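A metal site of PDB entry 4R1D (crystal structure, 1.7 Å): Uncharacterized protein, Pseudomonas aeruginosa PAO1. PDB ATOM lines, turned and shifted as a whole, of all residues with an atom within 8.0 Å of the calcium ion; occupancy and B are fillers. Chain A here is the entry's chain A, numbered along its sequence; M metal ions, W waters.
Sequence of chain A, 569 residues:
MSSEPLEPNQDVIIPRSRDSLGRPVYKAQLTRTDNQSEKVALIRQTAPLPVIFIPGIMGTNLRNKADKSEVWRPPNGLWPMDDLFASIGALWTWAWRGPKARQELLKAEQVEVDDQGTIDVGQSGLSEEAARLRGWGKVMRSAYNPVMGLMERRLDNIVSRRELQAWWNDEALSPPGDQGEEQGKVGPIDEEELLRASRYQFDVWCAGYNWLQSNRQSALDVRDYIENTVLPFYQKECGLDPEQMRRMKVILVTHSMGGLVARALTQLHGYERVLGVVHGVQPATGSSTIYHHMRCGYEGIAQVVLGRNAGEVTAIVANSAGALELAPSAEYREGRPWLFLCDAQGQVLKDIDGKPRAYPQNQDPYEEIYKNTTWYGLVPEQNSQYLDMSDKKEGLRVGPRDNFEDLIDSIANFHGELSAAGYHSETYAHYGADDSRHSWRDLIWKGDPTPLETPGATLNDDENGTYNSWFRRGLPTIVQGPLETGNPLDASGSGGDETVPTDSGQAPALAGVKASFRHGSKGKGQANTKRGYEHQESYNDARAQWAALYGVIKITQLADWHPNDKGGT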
ATOM      1  N   LEU A  49     -17.099  15.153 -12.068  1.00  0.00           N
ATOM      2  CA  LEU A  49     -18.484  14.742 -11.922  1.00  0.00           C
ATOM      3  C   LEU A  49     -18.504  13.222 -12.006  1.00  0.00           C
ATOM      4  O   LEU A  49     -18.585  12.655 -13.092  1.00  0.00           O
ATOM      5  CB  LEU A  49     -19.338  15.357 -13.046  1.00  0.00           C
ATOM      6  CG  LEU A  49     -20.857  15.242 -12.916  1.00  0.00           C
ATOM      7  CD1 LEU A  49     -21.273  15.592 -11.517  1.00  0.00           C
ATOM      8  CD2 LEU A  49     -21.590  16.146 -13.926  1.00  0.00           C
ATOM      9  N   SER A 124     -11.226   2.676 -23.282  1.00  0.00           N
ATOM     10  CA  SER A 124     -11.568   3.638 -22.236  1.00  0.00           C
ATOM     11  C   SER A 124     -10.503   4.703 -22.049  1.00  0.00           C
ATOM     12  O   SER A 124     -10.781   5.778 -21.516  1.00  0.00           O
ATOM     13  CB  SER A 124     -11.773   2.927 -20.895  1.00  0.00           C
ATOM     14  OG  SER A 124     -10.534   2.403 -20.426  1.00  0.00           O
ATOM     15  N   LEU A 126      -7.996   4.086 -20.122  1.00  0.00           N
ATOM     16  CA  LEU A 126      -7.504   3.802 -18.771  1.00  0.00           C
ATOM     17  C   LEU A 126      -6.520   2.646 -18.752  1.00  0.00           C
ATOM     18  O   LEU A 126      -6.699   1.680 -19.477  1.00  0.00           O
ATOM     19  CB  LEU A 126      -8.673   3.430 -17.840  1.00  0.00           C
ATOM     20  CG  LEU A 126      -9.684   4.509 -17.466  1.00  0.00           C
ATOM     21  CD1 LEU A 126     -10.761   3.933 -16.558  1.00  0.00           C
ATOM     22  CD2 LEU A 126      -8.979   5.672 -16.789  1.00  0.00           C
ATOM     23  N   ARG A 134     -10.686   2.013  -9.995  1.00  0.00           N
ATOM     24  CA  ARG A 134     -12.069   2.442 -10.200  1.00  0.00           C
ATOM     25  C   ARG A 134     -13.066   1.323  -9.919  1.00  0.00           C
ATOM     26  O   ARG A 134     -14.272   1.529 -10.042  1.00  0.00           O
ATOM     27  CB  ARG A 134     -12.293   2.921 -11.642  1.00  0.00           C
ATOM     28  CG  ARG A 134     -11.404   4.058 -12.098  1.00  0.00           C
ATOM     29  CD  ARG A 134     -11.973   5.404 -11.753  1.00  0.00           C
ATOM     30  NE  ARG A 134     -11.328   6.443 -12.557  1.00  0.00           N
ATOM     31  CZ  ARG A 134     -11.713   6.764 -13.789  1.00  0.00           C
ATOM     32  NH1 ARG A 134     -12.757   6.142 -14.342  1.00  0.00           N
ATOM     33  NH2 ARG A 134     -11.062   7.707 -14.462  1.00  0.00           N
ATOM     34  N   MET A 151     -18.713   4.886 -21.851  1.00  0.00           N
ATOM     35  CA  MET A 151     -19.109   6.117 -21.210  1.00  0.00           C
ATOM     36  C   MET A 151     -17.877   6.944 -20.863  1.00  0.00           C
ATOM     37  O   MET A 151     -17.864   8.175 -21.004  1.00  0.00           O
ATOM     38  CB  MET A 151     -19.937   5.824 -19.946  1.00  0.00           C
ATOM     39  CG  MET A 151     -21.292   5.221 -20.244  1.00  0.00           C
ATOM     40  SD  MET A 151     -22.364   5.182 -18.779  1.00  0.00           S
ATOM     41  CE  MET A 151     -21.485   3.996 -17.709  1.00  0.00           C
ATOM     42  N   GLU A 152     -16.838   6.272 -20.416  1.00  0.00           N
ATOM     43  CA  GLU A 152     -15.615   6.977 -20.031  1.00  0.00           C
ATOM     44  C   GLU A 152     -15.044   7.736 -21.236  1.00  0.00           C
ATOM     45  O   GLU A 152     -14.737   8.928 -21.136  1.00  0.00           O
ATOM     46  CB  GLU A 152     -14.577   5.990 -19.480  1.00  0.00           C
ATOM     47  CG  GLU A 152     -13.325   6.652 -18.919  1.00  0.00           C
ATOM     48  CD  GLU A 152     -13.467   7.064 -17.470  1.00  0.00           C
ATOM     49  OE1 GLU A 152     -14.261   6.465 -16.729  1.00  0.00           O
ATOM     50  OE2 GLU A 152     -12.787   8.010 -17.046  1.00  0.00           O
ATOM     51  N   ARG A 153     -14.896   7.045 -22.364  1.00  0.00           N
ATOM     52  CA  ARG A 153     -14.301   7.698 -23.538  1.00  0.00           C
ATOM     53  C   ARG A 153     -15.243   8.723 -24.143  1.00  0.00           C
ATOM     54  O   ARG A 153     -14.811   9.813 -24.553  1.00  0.00           O
ATOM     55  CB  ARG A 153     -13.825   6.691 -24.590  1.00  0.00           C
ATOM     56  CG  ARG A 153     -14.867   5.893 -25.349  1.00  0.00           C
ATOM     57  CD  ARG A 153     -14.157   5.000 -26.402  1.00  0.00           C
ATOM     58  NE  ARG A 153     -15.101   4.305 -27.268  1.00  0.00           N
ATOM     59  CZ  ARG A 153     -15.410   4.693 -28.500  1.00  0.00           C
ATOM     60  NH1 ARG A 153     -14.838   5.771 -29.039  1.00  0.00           N
ATOM     61  NH2 ARG A 153     -16.286   4.000 -29.217  1.00  0.00           N
ATOM     62  N   LEU A 155     -17.615  10.467 -22.584  1.00  0.00           N
ATOM     63  CA  LEU A 155     -17.758  11.643 -21.717  1.00  0.00           C
ATOM     64  C   LEU A 155     -16.459  12.460 -21.595  1.00  0.00           C
ATOM     65  O   LEU A 155     -16.496  13.630 -21.220  1.00  0.00           O
ATOM     66  CB  LEU A 155     -18.309  11.254 -20.339  1.00  0.00           C
ATOM     67  CG  LEU A 155     -19.734  10.673 -20.386  1.00  0.00           C
ATOM     68  CD1 LEU A 155     -20.088   9.980 -19.073  1.00  0.00           C
ATOM     69  CD2 LEU A 155     -20.762  11.769 -20.708  1.00  0.00           C
ATOM     70  N   ASP A 156     -15.339  11.817 -21.916  1.00  0.00           N
ATOM     71  CA  ASP A 156     -14.028  12.468 -21.913  1.00  0.00           C
ATOM     72  C   ASP A 156     -13.764  13.156 -23.265  1.00  0.00           C
ATOM     73  O   ASP A 156     -12.752  13.821 -23.437  1.00  0.00           O
ATOM     74  CB  ASP A 156     -12.918  11.441 -21.657  1.00  0.00           C
ATOM     75  CG  ASP A 156     -12.812  11.044 -20.202  1.00  0.00           C
ATOM     76  OD1 ASP A 156     -13.492  11.679 -19.361  1.00  0.00           O
ATOM     77  OD2 ASP A 156     -12.038  10.094 -19.877  1.00  0.00           O
ATOM     78  N   ASN A 157     -14.684  12.979 -24.205  1.00  0.00           N
ATOM     79  CA  ASN A 157     -14.507  13.500 -25.548  1.00  0.00           C
ATOM     80  C   ASN A 157     -15.789  14.091 -26.133  1.00  0.00           C
ATOM     81  O   ASN A 157     -16.279  13.607 -27.151  1.00  0.00           O
ATOM     82  CB  ASN A 157     -13.981  12.395 -26.466  1.00  0.00           C
ATOM     83  CG  ASN A 157     -12.553  11.988 -26.120  1.00  0.00           C
ATOM     84  OD1 ASN A 157     -11.598  12.672 -26.502  1.00  0.00           O
ATOM     85  ND2 ASN A 157     -12.407  10.899 -25.365  1.00  0.00           N
ATOM     86  N   TYR A 200     -17.243  19.635 -17.574  1.00  0.00           N
ATOM     87  CA  TYR A 200     -17.018  18.710 -16.467  1.00  0.00           C
ATOM     88  C   TYR A 200     -16.118  17.543 -16.851  1.00  0.00           C
ATOM     89  O   TYR A 200     -16.083  17.146 -18.002  1.00  0.00           O
ATOM     90  CB  TYR A 200     -18.350  18.165 -15.951  1.00  0.00           C
ATOM     91  CG  TYR A 200     -19.239  19.222 -15.372  1.00  0.00           C
ATOM     92  CD1 TYR A 200     -19.185  19.554 -14.027  1.00  0.00           C
ATOM     93  CD2 TYR A 200     -20.126  19.914 -16.184  1.00  0.00           C
ATOM     94  CE1 TYR A 200     -20.007  20.535 -13.501  1.00  0.00           C
ATOM     95  CE2 TYR A 200     -20.950  20.891 -15.675  1.00  0.00           C
ATOM     96  CZ  TYR A 200     -20.886  21.202 -14.336  1.00  0.00           C
ATOM     97  OH  TYR A 200     -21.712  22.169 -13.830  1.00  0.00           O
ATOM     98  N   GLN A 201     -15.391  17.008 -15.874  1.00  0.00           N
ATOM     99  CA  GLN A 201     -14.601  15.799 -16.100  1.00  0.00           C
ATOM    100  C   GLN A 201     -15.329  14.598 -15.504  1.00  0.00           C
ATOM    101  O   GLN A 201     -15.442  14.469 -14.278  1.00  0.00           O
ATOM    102  CB  GLN A 201     -13.198  15.920 -15.498  1.00  0.00           C
ATOM    103  CG  GLN A 201     -12.332  17.010 -16.131  1.00  0.00           C
ATOM    104  CD  GLN A 201     -12.701  18.416 -15.681  1.00  0.00           C
ATOM    105  OE1 GLN A 201     -13.369  18.582 -14.661  1.00  0.00           O
ATOM    106  NE2 GLN A 201     -12.283  19.422 -16.439  1.00  0.00           N
ATOM    107  N   PHE A 202     -15.836  13.729 -16.370  1.00  0.00           N
ATOM    108  CA  PHE A 202     -16.578  12.569 -15.903  1.00  0.00           C
ATOM    109  C   PHE A 202     -15.595  11.425 -15.737  1.00  0.00           C
ATOM    110  O   PHE A 202     -14.708  11.242 -16.550  1.00  0.00           O
ATOM    111  CB  PHE A 202     -17.644  12.174 -16.918  1.00  0.00           C
ATOM    112  CG  PHE A 202     -18.655  13.247 -17.194  1.00  0.00           C
ATOM    113  CD1 PHE A 202     -19.860  13.286 -16.503  1.00  0.00           C
ATOM    114  CD2 PHE A 202     -18.399  14.237 -18.144  1.00  0.00           C
ATOM    115  CE1 PHE A 202     -20.796  14.279 -16.765  1.00  0.00           C
ATOM    116  CE2 PHE A 202     -19.329  15.225 -18.400  1.00  0.00           C
ATOM    117  CZ  PHE A 202     -20.525  15.242 -17.715  1.00  0.00           C
ATOM    118  N   ASP A 203     -15.754  10.659 -14.662  1.00  0.00           N
ATOM    119  CA  ASP A 203     -14.996   9.431 -14.438  1.00  0.00           C
ATOM    120  C   ASP A 203     -15.984   8.363 -13.979  1.00  0.00           C
ATOM    121  O   ASP A 203     -16.813   8.624 -13.096  1.00  0.00           O
ATOM    122  CB  ASP A 203     -13.977   9.611 -13.316  1.00  0.00           C
ATOM    123  CG  ASP A 203     -12.772  10.446 -13.722  1.00  0.00           C
ATOM    124  OD1 ASP A 203     -12.415  10.473 -14.913  1.00  0.00           O
ATOM    125  OD2 ASP A 203     -12.157  11.051 -12.823  1.00  0.00           O
ATOM    126  N   VAL A 204     -15.894   7.160 -14.536  1.00  0.00           N
ATOM    127  CA  VAL A 204     -16.812   6.085 -14.165  1.00  0.00           C
ATOM    128  C   VAL A 204     -16.215   5.215 -13.062  1.00  0.00           C
ATOM    129  O   VAL A 204     -15.150   4.634 -13.244  1.00  0.00           O
ATOM    130  CB  VAL A 204     -17.130   5.181 -15.360  1.00  0.00           C
ATOM    131  CG1 VAL A 204     -18.114   4.074 -14.946  1.00  0.00           C
ATOM    132  CG2 VAL A 204     -17.711   6.008 -16.537  1.00  0.00           C
ATOM    133  N   TRP A 205     -16.927   5.121 -11.936  1.00  0.00           N
ATOM    134  CA  TRP A 205     -16.513   4.302 -10.807  1.00  0.00           C
ATOM    135  C   TRP A 205     -17.518   3.167 -10.683  1.00  0.00           C
ATOM    136  O   TRP A 205     -18.689   3.352 -10.976  1.00  0.00           O
ATOM    137  CB  TRP A 205     -16.494   5.117  -9.515  1.00  0.00           C
ATOM    138  CG  TRP A 205     -15.440   6.186  -9.532  1.00  0.00           C
ATOM    139  CD1 TRP A 205     -15.492   7.374 -10.206  1.00  0.00           C
ATOM    140  CD2 TRP A 205     -14.198   6.159  -8.836  1.00  0.00           C
ATOM    141  NE1 TRP A 205     -14.347   8.098  -9.963  1.00  0.00           N
ATOM    142  CE2 TRP A 205     -13.526   7.374  -9.138  1.00  0.00           C
ATOM    143  CE3 TRP A 205     -13.561   5.235  -7.992  1.00  0.00           C
ATOM    144  CZ2 TRP A 205     -12.265   7.684  -8.613  1.00  0.00           C
ATOM    145  CZ3 TRP A 205     -12.314   5.548  -7.467  1.00  0.00           C
ATOM    146  CH2 TRP A 205     -11.680   6.761  -7.795  1.00  0.00           C
ATOM    147  N   TYR A 234     -10.871  12.502  -5.190  1.00  0.00           N
ATOM    148  CA  TYR A 234     -10.874  13.844  -5.783  1.00  0.00           C
ATOM    149  C   TYR A 234     -10.418  14.895  -4.780  1.00  0.00           C
ATOM    150  O   TYR A 234      -9.748  15.860  -5.149  1.00  0.00           O
ATOM    151  CB  TYR A 234     -12.254  14.201  -6.377  1.00  0.00           C
ATOM    152  CG  TYR A 234     -12.573  13.291  -7.529  1.00  0.00           C
ATOM    153  CD1 TYR A 234     -11.976  13.484  -8.771  1.00  0.00           C
ATOM    154  CD2 TYR A 234     -13.430  12.215  -7.372  1.00  0.00           C
ATOM    155  CE1 TYR A 234     -12.241  12.635  -9.829  1.00  0.00           C
ATOM    156  CE2 TYR A 234     -13.702  11.366  -8.424  1.00  0.00           C
ATOM    157  CZ  TYR A 234     -13.112  11.584  -9.642  1.00  0.00           C
ATOM    158  OH  TYR A 234     -13.388  10.720 -10.684  1.00  0.00           O
HETATM  159 CA    CA M   1     -12.634  10.402 -17.375  1.00  0.00          CA
HETATM  160  O   HOH W   1     -11.387  12.710 -17.072  1.00  0.00           O
HETATM  161  O   HOH W   2     -10.208   9.569 -17.108  1.00  0.00           O
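The calcium ion is bound by the backbone carbonyl oxygen (O) of Phe 202, the side-chain carboxylate (OE2) of Glu 152, the side-chain carboxylate (OD1) of Asp 203, the side-chain carboxylate (OD1) of Asp 156, water W2, the side-chain carboxylate (OD2) of Asp 156 and water W1.
Four residues have an atom within 4 Å of the calcium ion: Glu 152, Asp 156, Phe 202 and Asp 203. The nearest printed residue that does not touch the calcium ion is Arg 134 (4.3 Å).
The side-chain hydroxyl of Tyr 234 lies within hydrogen-bond range of the side-chain carboxylate of Asp 203 (2.5 Å). NH1 of Arg 134 is in salt-bridge range of OE1 of Glu 152 (2.8 Å). The side-chain carboxylate (OE1) of Glu 152 is in hydrogen-bond range of the backbone NH (N) of Val 204. OD2 of Asp 203 lies within salt-bridge range of NH2 of Arg 134.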
